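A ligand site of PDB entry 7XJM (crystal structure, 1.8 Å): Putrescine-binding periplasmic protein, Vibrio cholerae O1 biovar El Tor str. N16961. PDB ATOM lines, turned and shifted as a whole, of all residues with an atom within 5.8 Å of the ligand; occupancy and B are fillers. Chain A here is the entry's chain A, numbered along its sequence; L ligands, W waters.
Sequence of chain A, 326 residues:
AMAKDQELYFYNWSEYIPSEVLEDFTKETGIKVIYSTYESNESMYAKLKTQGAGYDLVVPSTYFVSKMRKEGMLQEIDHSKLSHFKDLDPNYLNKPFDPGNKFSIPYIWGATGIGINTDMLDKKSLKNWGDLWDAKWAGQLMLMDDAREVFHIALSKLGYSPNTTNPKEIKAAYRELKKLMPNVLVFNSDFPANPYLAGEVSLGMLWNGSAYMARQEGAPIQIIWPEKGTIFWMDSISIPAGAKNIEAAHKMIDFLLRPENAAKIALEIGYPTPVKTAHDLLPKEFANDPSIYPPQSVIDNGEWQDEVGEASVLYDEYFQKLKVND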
ATOM      1  N   TRP A  13      -2.070 -20.275   5.177  1.00  0.00           N
ATOM      2  CA  TRP A  13      -0.990 -19.847   4.286  1.00  0.00           C
ATOM      3  C   TRP A  13       0.072 -20.926   4.261  1.00  0.00           C
ATOM      4  O   TRP A  13       0.304 -21.595   5.283  1.00  0.00           O
ATOM      5  CB  TRP A  13      -0.358 -18.545   4.798  1.00  0.00           C
ATOM      6  CG  TRP A  13      -1.304 -17.374   4.793  1.00  0.00           C
ATOM      7  CD1 TRP A  13      -2.251 -17.076   5.731  1.00  0.00           C
ATOM      8  CD2 TRP A  13      -1.464 -16.403   3.756  1.00  0.00           C
ATOM      9  NE1 TRP A  13      -2.930 -15.931   5.382  1.00  0.00           N
ATOM     10  CE2 TRP A  13      -2.473 -15.504   4.167  1.00  0.00           C
ATOM     11  CE3 TRP A  13      -0.785 -16.157   2.548  1.00  0.00           C
ATOM     12  CZ2 TRP A  13      -2.878 -14.411   3.370  1.00  0.00           C
ATOM     13  CZ3 TRP A  13      -1.181 -15.066   1.773  1.00  0.00           C
ATOM     14  CH2 TRP A  13      -2.210 -14.207   2.191  1.00  0.00           C
ATOM     15  N   SER A  14       0.761 -21.056   3.129  1.00  0.00           N
ATOM     16  CA  SER A  14       1.900 -21.961   3.039  1.00  0.00           C
ATOM     17  C   SER A  14       2.960 -21.445   4.020  1.00  0.00           C
ATOM     18  O   SER A  14       2.906 -20.288   4.429  1.00  0.00           O
ATOM     19  CB  SER A  14       2.475 -21.935   1.626  1.00  0.00           C
ATOM     20  OG  SER A  14       2.940 -20.635   1.284  1.00  0.00           O
ATOM     21  N   GLU A  15       3.907 -22.321   4.412  1.00  0.00           N
ATOM     22  CA  GLU A  15       5.106 -22.033   5.240  1.00  0.00           C
ATOM     23  C   GLU A  15       4.904 -21.701   6.715  1.00  0.00           C
ATOM     24  O   GLU A  15       5.896 -21.700   7.444  1.00  0.00           O
ATOM     25  CB  GLU A  15       5.931 -20.881   4.622  1.00  0.00           C
ATOM     26  CG  GLU A  15       6.124 -21.015   3.114  1.00  0.00           C
ATOM     27  CD  GLU A  15       6.816 -19.824   2.497  1.00  0.00           C
ATOM     28  OE1 GLU A  15       7.874 -20.049   1.892  1.00  0.00           O
ATOM     29  OE2 GLU A  15       6.312 -18.680   2.599  1.00  0.00           O
ATOM     30  N   TYR A  16       3.689 -21.399   7.172  1.00  0.00           N
ATOM     31  CA  TYR A  16       3.447 -21.002   8.567  1.00  0.00           C
ATOM     32  C   TYR A  16       3.576 -22.099   9.595  1.00  0.00           C
ATOM     33  O   TYR A  16       4.061 -21.823  10.707  1.00  0.00           O
ATOM     34  CB  TYR A  16       2.069 -20.346   8.706  1.00  0.00           C
ATOM     35  CG  TYR A  16       1.999 -18.853   8.399  1.00  0.00           C
ATOM     36  CD1 TYR A  16       3.154 -18.063   8.397  1.00  0.00           C
ATOM     37  CD2 TYR A  16       0.760 -18.219   8.231  1.00  0.00           C
ATOM     38  CE1 TYR A  16       3.078 -16.680   8.186  1.00  0.00           C
ATOM     39  CE2 TYR A  16       0.690 -16.848   7.990  1.00  0.00           C
ATOM     40  CZ  TYR A  16       1.842 -16.080   7.970  1.00  0.00           C
ATOM     41  OH  TYR A  16       1.740 -14.723   7.795  1.00  0.00           O
ATOM     42  N   ASN A  41      -4.857 -14.336  -0.158  1.00  0.00           N
ATOM     43  CA  ASN A  41      -6.242 -14.187   0.321  1.00  0.00           C
ATOM     44  C   ASN A  41      -7.190 -14.428  -0.847  1.00  0.00           C
ATOM     45  O   ASN A  41      -8.269 -14.964  -0.652  1.00  0.00           O
ATOM     46  CB  ASN A  41      -6.475 -12.756   0.815  1.00  0.00           C
ATOM     47  CG  ASN A  41      -5.794 -12.465   2.137  1.00  0.00           C
ATOM     48  OD1 ASN A  41      -6.225 -12.962   3.177  1.00  0.00           O
ATOM     49  ND2 ASN A  41      -4.701 -11.712   2.079  1.00  0.00           N
ATOM     50  N   SER A  61      -5.962 -12.288   5.931  1.00  0.00           N
ATOM     51  CA  SER A  61      -5.246 -11.095   6.347  1.00  0.00           C
ATOM     52  C   SER A  61      -6.349 -10.156   6.871  1.00  0.00           C
ATOM     53  O   SER A  61      -7.520 -10.303   6.509  1.00  0.00           O
ATOM     54  CB  SER A  61      -4.529 -10.436   5.176  1.00  0.00           C
ATOM     55  OG  SER A  61      -3.511 -11.270   4.653  1.00  0.00           O
ATOM     56  N   TYR A  63      -7.297  -7.252   6.137  1.00  0.00           N
ATOM     57  CA  TYR A  63      -8.029  -6.521   5.109  1.00  0.00           C
ATOM     58  C   TYR A  63      -9.090  -7.376   4.382  1.00  0.00           C
ATOM     59  O   TYR A  63      -9.790  -6.857   3.509  1.00  0.00           O
ATOM     60  CB  TYR A  63      -7.072  -5.813   4.122  1.00  0.00           C
ATOM     61  CG  TYR A  63      -6.132  -6.704   3.352  1.00  0.00           C
ATOM     62  CD1 TYR A  63      -6.453  -7.153   2.062  1.00  0.00           C
ATOM     63  CD2 TYR A  63      -4.861  -6.997   3.838  1.00  0.00           C
ATOM     64  CE1 TYR A  63      -5.556  -7.911   1.309  1.00  0.00           C
ATOM     65  CE2 TYR A  63      -3.952  -7.744   3.102  1.00  0.00           C
ATOM     66  CZ  TYR A  63      -4.307  -8.207   1.836  1.00  0.00           C
ATOM     67  OH  TYR A  63      -3.394  -8.933   1.119  1.00  0.00           O
ATOM     68  N   ASP A 146       0.425 -11.396  -5.292  1.00  0.00           N
ATOM     69  CA  ASP A 146      -0.565 -10.813  -4.404  1.00  0.00           C
ATOM     70  C   ASP A 146      -1.009  -9.470  -4.984  1.00  0.00           C
ATOM     71  O   ASP A 146      -0.199  -8.553  -5.073  1.00  0.00           O
ATOM     72  CB  ASP A 146       0.125 -10.606  -3.030  1.00  0.00           C
ATOM     73  CG  ASP A 146      -0.811 -10.222  -1.911  1.00  0.00           C
ATOM     74  OD1 ASP A 146      -1.419  -9.134  -2.010  1.00  0.00           O
ATOM     75  OD2 ASP A 146      -0.908 -11.004  -0.926  1.00  0.00           O
ATOM     76  N   ARG A 148      -2.943  -6.949  -3.902  1.00  0.00           N
ATOM     77  CA  ARG A 148      -2.828  -5.747  -3.072  1.00  0.00           C
ATOM     78  C   ARG A 148      -1.402  -5.355  -2.801  1.00  0.00           C
ATOM     79  O   ARG A 148      -1.124  -4.148  -2.782  1.00  0.00           O
ATOM     80  CB  ARG A 148      -3.624  -5.877  -1.771  1.00  0.00           C
ATOM     81  CG  ARG A 148      -5.152  -5.997  -2.035  1.00  0.00           C
ATOM     82  CD  ARG A 148      -5.818  -4.718  -2.598  1.00  0.00           C
ATOM     83  NE  ARG A 148      -5.381  -3.517  -1.879  1.00  0.00           N
ATOM     84  CZ  ARG A 148      -5.729  -3.219  -0.633  1.00  0.00           C
ATOM     85  NH1 ARG A 148      -6.573  -4.003   0.028  1.00  0.00           N
ATOM     86  NH2 ARG A 148      -5.240  -2.145  -0.037  1.00  0.00           N
ATOM     87  N   GLU A 149      -0.482  -6.317  -2.642  1.00  0.00           N
ATOM     88  CA  GLU A 149       0.912  -5.942  -2.400  1.00  0.00           C
ATOM     89  C   GLU A 149       1.544  -5.348  -3.655  1.00  0.00           C
ATOM     90  O   GLU A 149       2.263  -4.355  -3.553  1.00  0.00           O
ATOM     91  CB  GLU A 149       1.732  -7.137  -1.929  1.00  0.00           C
ATOM     92  CG  GLU A 149       1.390  -7.604  -0.536  1.00  0.00           C
ATOM     93  CD  GLU A 149       2.502  -8.392   0.140  1.00  0.00           C
ATOM     94  OE1 GLU A 149       3.675  -8.120  -0.169  1.00  0.00           O
ATOM     95  OE2 GLU A 149       2.202  -9.249   0.997  1.00  0.00           O
ATOM     96  N   SER A 189       4.177 -16.222  -4.218  1.00  0.00           N
ATOM     97  CA  SER A 189       3.850 -15.994  -2.795  1.00  0.00           C
ATOM     98  C   SER A 189       3.766 -17.358  -2.086  1.00  0.00           C
ATOM     99  O   SER A 189       3.466 -17.411  -0.887  1.00  0.00           O
ATOM    100  CB  SER A 189       2.517 -15.266  -2.661  1.00  0.00           C
ATOM    101  OG  SER A 189       2.656 -13.874  -2.877  1.00  0.00           O
ATOM    102  N   ASP A 190       4.007 -18.444  -2.832  1.00  0.00           N
ATOM    103  CA  ASP A 190       3.909 -19.781  -2.271  1.00  0.00           C
ATOM    104  C   ASP A 190       5.163 -20.227  -1.494  1.00  0.00           C
ATOM    105  O   ASP A 190       5.038 -20.836  -0.434  1.00  0.00           O
ATOM    106  CB  ASP A 190       3.580 -20.787  -3.358  1.00  0.00           C
ATOM    107  CG  ASP A 190       2.887 -22.050  -2.853  1.00  0.00           C
ATOM    108  OD1 ASP A 190       2.731 -22.194  -1.618  1.00  0.00           O
ATOM    109  OD2 ASP A 190       2.499 -22.866  -3.692  1.00  0.00           O
ATOM    110  N   PRO A 192       8.380 -17.990  -1.619  1.00  0.00           N
ATOM    111  CA  PRO A 192       9.138 -16.872  -2.227  1.00  0.00           C
ATOM    112  C   PRO A 192      10.639 -16.809  -1.925  1.00  0.00           C
ATOM    113  O   PRO A 192      11.349 -16.230  -2.728  1.00  0.00           O
ATOM    114  CB  PRO A 192       8.401 -15.615  -1.735  1.00  0.00           C
ATOM    115  CG  PRO A 192       7.709 -16.030  -0.514  1.00  0.00           C
ATOM    116  CD  PRO A 192       7.316 -17.457  -0.748  1.00  0.00           C
ATOM    117  N   TRP A 207       8.994 -10.982   1.659  1.00  0.00           N
ATOM    118  CA  TRP A 207       8.490 -10.937   3.019  1.00  0.00           C
ATOM    119  C   TRP A 207       9.679 -11.077   3.976  1.00  0.00           C
ATOM    120  O   TRP A 207      10.630 -11.824   3.670  1.00  0.00           O
ATOM    121  CB  TRP A 207       7.519 -12.085   3.276  1.00  0.00           C
ATOM    122  CG  TRP A 207       6.177 -11.926   2.630  1.00  0.00           C
ATOM    123  CD1 TRP A 207       5.484 -10.758   2.464  1.00  0.00           C
ATOM    124  CD2 TRP A 207       5.345 -12.969   2.126  1.00  0.00           C
ATOM    125  NE1 TRP A 207       4.285 -11.011   1.836  1.00  0.00           N
ATOM    126  CE2 TRP A 207       4.173 -12.358   1.623  1.00  0.00           C
ATOM    127  CE3 TRP A 207       5.510 -14.361   1.970  1.00  0.00           C
ATOM    128  CZ2 TRP A 207       3.139 -13.099   1.033  1.00  0.00           C
ATOM    129  CZ3 TRP A 207       4.497 -15.091   1.363  1.00  0.00           C
ATOM    130  CH2 TRP A 207       3.326 -14.461   0.892  1.00  0.00           C
ATOM    131  N   SER A 210      10.414 -14.799   4.927  1.00  0.00           N
ATOM    132  CA  SER A 210      11.029 -15.547   3.829  1.00  0.00           C
ATOM    133  C   SER A 210      12.527 -15.236   3.733  1.00  0.00           C
ATOM    134  O   SER A 210      13.329 -16.162   3.576  1.00  0.00           O
ATOM    135  CB  SER A 210      10.331 -15.219   2.500  1.00  0.00           C
ATOM    136  OG  SER A 210       8.934 -15.454   2.576  1.00  0.00           O
ATOM    137  N   ILE A 231       5.344  -2.274   3.192  1.00  0.00           N
ATOM    138  CA  ILE A 231       4.067  -2.949   3.409  1.00  0.00           C
ATOM    139  C   ILE A 231       4.060  -3.632   4.765  1.00  0.00           C
ATOM    140  O   ILE A 231       4.956  -4.421   5.044  1.00  0.00           O
ATOM    141  CB  ILE A 231       3.758  -3.992   2.275  1.00  0.00           C
ATOM    142  CG1 ILE A 231       4.000  -3.422   0.845  1.00  0.00           C
ATOM    143  CG2 ILE A 231       2.324  -4.537   2.425  1.00  0.00           C
ATOM    144  CD1 ILE A 231       3.778  -4.457  -0.337  1.00  0.00           C
ATOM    145  N   TRP A 233       1.441  -6.021   7.268  1.00  0.00           N
ATOM    146  CA  TRP A 233       0.226  -6.834   7.209  1.00  0.00           C
ATOM    147  C   TRP A 233       0.120  -7.754   8.400  1.00  0.00           C
ATOM    148  O   TRP A 233       1.118  -8.018   9.086  1.00  0.00           O
ATOM    149  CB  TRP A 233       0.126  -7.647   5.889  1.00  0.00           C
ATOM    150  CG  TRP A 233       1.418  -8.339   5.512  1.00  0.00           C
ATOM    151  CD1 TRP A 233       2.310  -7.920   4.579  1.00  0.00           C
ATOM    152  CD2 TRP A 233       1.964  -9.537   6.091  1.00  0.00           C
ATOM    153  NE1 TRP A 233       3.398  -8.769   4.544  1.00  0.00           N
ATOM    154  CE2 TRP A 233       3.210  -9.778   5.460  1.00  0.00           C
ATOM    155  CE3 TRP A 233       1.532 -10.442   7.092  1.00  0.00           C
ATOM    156  CZ2 TRP A 233       4.006 -10.888   5.769  1.00  0.00           C
ATOM    157  CZ3 TRP A 233       2.305 -11.560   7.362  1.00  0.00           C
ATOM    158  CH2 TRP A 233       3.537 -11.757   6.736  1.00  0.00           C
ATOM    159  N   ASP A 235      -2.007 -11.479   9.594  1.00  0.00           N
ATOM    160  CA  ASP A 235      -2.866 -12.632   9.322  1.00  0.00           C
ATOM    161  C   ASP A 235      -3.494 -13.052  10.635  1.00  0.00           C
ATOM    162  O   ASP A 235      -2.824 -13.065  11.690  1.00  0.00           O
ATOM    163  CB  ASP A 235      -2.059 -13.766   8.706  1.00  0.00           C
ATOM    164  CG  ASP A 235      -1.647 -13.485   7.275  1.00  0.00           C
ATOM    165  OD1 ASP A 235      -2.390 -12.756   6.569  1.00  0.00           O
ATOM    166  OD2 ASP A 235      -0.579 -13.967   6.859  1.00  0.00           O
ATOM    167  N   TYR A 271       9.033 -14.947  11.265  1.00  0.00           N
ATOM    168  CA  TYR A 271       8.077 -13.871  11.374  1.00  0.00           C
ATOM    169  C   TYR A 271       7.878 -13.376  12.789  1.00  0.00           C
ATOM    170  O   TYR A 271       7.850 -14.186  13.719  1.00  0.00           O
ATOM    171  CB  TYR A 271       6.701 -14.293  10.801  1.00  0.00           C
ATOM    172  CG  TYR A 271       6.706 -14.420   9.296  1.00  0.00           C
ATOM    173  CD1 TYR A 271       6.618 -13.289   8.473  1.00  0.00           C
ATOM    174  CD2 TYR A 271       6.816 -15.657   8.685  1.00  0.00           C
ATOM    175  CE1 TYR A 271       6.648 -13.401   7.089  1.00  0.00           C
ATOM    176  CE2 TYR A 271       6.856 -15.779   7.300  1.00  0.00           C
ATOM    177  CZ  TYR A 271       6.765 -14.652   6.504  1.00  0.00           C
ATOM    178  OH  TYR A 271       6.821 -14.770   5.143  1.00  0.00           O
ATOM    179  N   GLN A 305      -1.747  -2.717   5.331  1.00  0.00           N
ATOM    180  CA  GLN A 305      -2.699  -3.057   4.268  1.00  0.00           C
ATOM    181  C   GLN A 305      -4.090  -3.031   4.892  1.00  0.00           C
ATOM    182  O   GLN A 305      -4.348  -3.693   5.908  1.00  0.00           O
ATOM    183  CB  GLN A 305      -2.406  -4.434   3.667  1.00  0.00           C
ATOM    184  CG  GLN A 305      -1.043  -4.495   3.012  1.00  0.00           C
ATOM    185  CD  GLN A 305      -0.989  -5.601   1.985  1.00  0.00           C
ATOM    186  OE1 GLN A 305      -0.706  -6.749   2.321  1.00  0.00           O
ATOM    187  NE2 GLN A 305      -1.259  -5.273   0.721  1.00  0.00           N
HETATM  188  N1  LIG L   1       3.755 -17.771   3.551  1.00  0.00           N
HETATM  189  C1  LIG L   1       3.727 -17.067   4.846  1.00  0.00           C
HETATM  190  C2  LIG L   1       3.536 -15.555   4.724  1.00  0.00           C
HETATM  191  C3  LIG L   1       2.063 -15.194   4.458  1.00  0.00           C
HETATM  192  C4  LIG L   1       1.766 -13.697   4.373  1.00  0.00           C
HETATM  193  N2  LIG L   1       0.331 -13.447   4.251  1.00  0.00           N
HETATM  194  C5  LIG L   1      -0.042 -12.026   4.246  1.00  0.00           C
HETATM  195  C6  LIG L   1       0.051 -11.397   2.861  1.00  0.00           C
HETATM  196  C7  LIG L   1      -0.529  -9.993   2.803  1.00  0.00           C
HETATM  197  N3  LIG L   1      -0.455  -9.433   1.470  1.00  0.00           N
HETATM  198  O   HOH W   1       2.022 -17.944   1.361  1.00  0.00           O
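The side-chain carboxylate (OE2) of Glu 149 lies within salt-bridge range of a nitrogen (N3) of the ligand, at 2.7 Å. O of Ser 14 is in hydrogen-bond range of N1 of the ligand (2.8 Å). OD2 of Asp 235 lies within salt-bridge range of N2 of the ligand, at 2.8 Å. OE1 of Gln 305 lies within hydrogen-bond range of N3 of the ligand, at 2.8 Å. A nitrogen (N1) of the ligand lies within salt-bridge range of the side-chain carboxylate (OE2) of Glu 15 (2.9 Å). A nitrogen (N3) of the ligand lies within salt-bridge range of the side-chain carboxylate (OD2) of Asp 146 (2.9 Å). N3 of the ligand sits at hydrogen-bond distance from OH of Tyr 63 (3.0 Å).
The side-chain carboxylate (OE2) of Glu 149 sits at hydrogen-bond distance from the indole nitrogen (NE1) of Trp 207 (2.9 Å). The side-chain hydroxyl (OG) of Ser 14 is in hydrogen-bond range of the backbone carbonyl oxygen (O) of Asp 190 (2.7 Å). The side-chain carboxylate (OD2) of Asp 235 sits close to the indole nitrogen (NE1) of Trp 13, 3.4 Å away. OG of Ser 61 sits at hydrogen-bond distance from OD1 of Asp 235 (2.7 Å). The side-chain carboxylate (OD1) of Asp 146 lies within hydrogen-bond range of the backbone NH (N) of Arg 148, 3.3 Å away. The side-chain amide nitrogen (ND2) of Asn 41 sits at hydrogen-bond distance from the side-chain hydroxyl (OH) of Tyr 63. The side-chain hydroxyl (OH) of Tyr 271 sits at hydrogen-bond distance from the side-chain hydroxyl (OG) of Ser 210, at 3.4 Å. The side-chain amide oxygen of Asn 41 sits at hydrogen-bond distance from the backbone NH of Ser 61 (2.8 Å).
Trp 13 touches the ligand. Tyr 16 touches the ligand (OH to C3, 3.4 Å). OG of Ser 61 touches C5 of the ligand, 3.6 Å away. Trp 207 touches the ligand (CZ3 to C2, 3.5 Å). CH2 of Trp 233 touches C4 of the ligand, at 3.5 Å. Tyr 271 touches the ligand. Hydrophobic or aromatic side chains that line the ligand: Trp 13, Tyr 16, Trp 207, Trp 233 and Tyr 271. Within 4 Å of the ligand: Trp 13, Ser 14, Glu 15, Tyr 16, Ser 61, Tyr 63, Asp 146, Glu 149, Trp 207, Trp 233, Asp 235, Tyr 271 and Gln 305. The nearest printed residue that does not touch the ligand is Ser 189 (4.5 Å).
Water W1 lies within hydrogen-bond range of the backbone carbonyl oxygen (O) of Ser 189 (2.7 Å), a nitrogen (N1) of the ligand (2.8 Å) and the side-chain hydroxyl (OG) of Ser 14 (2.8 Å).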
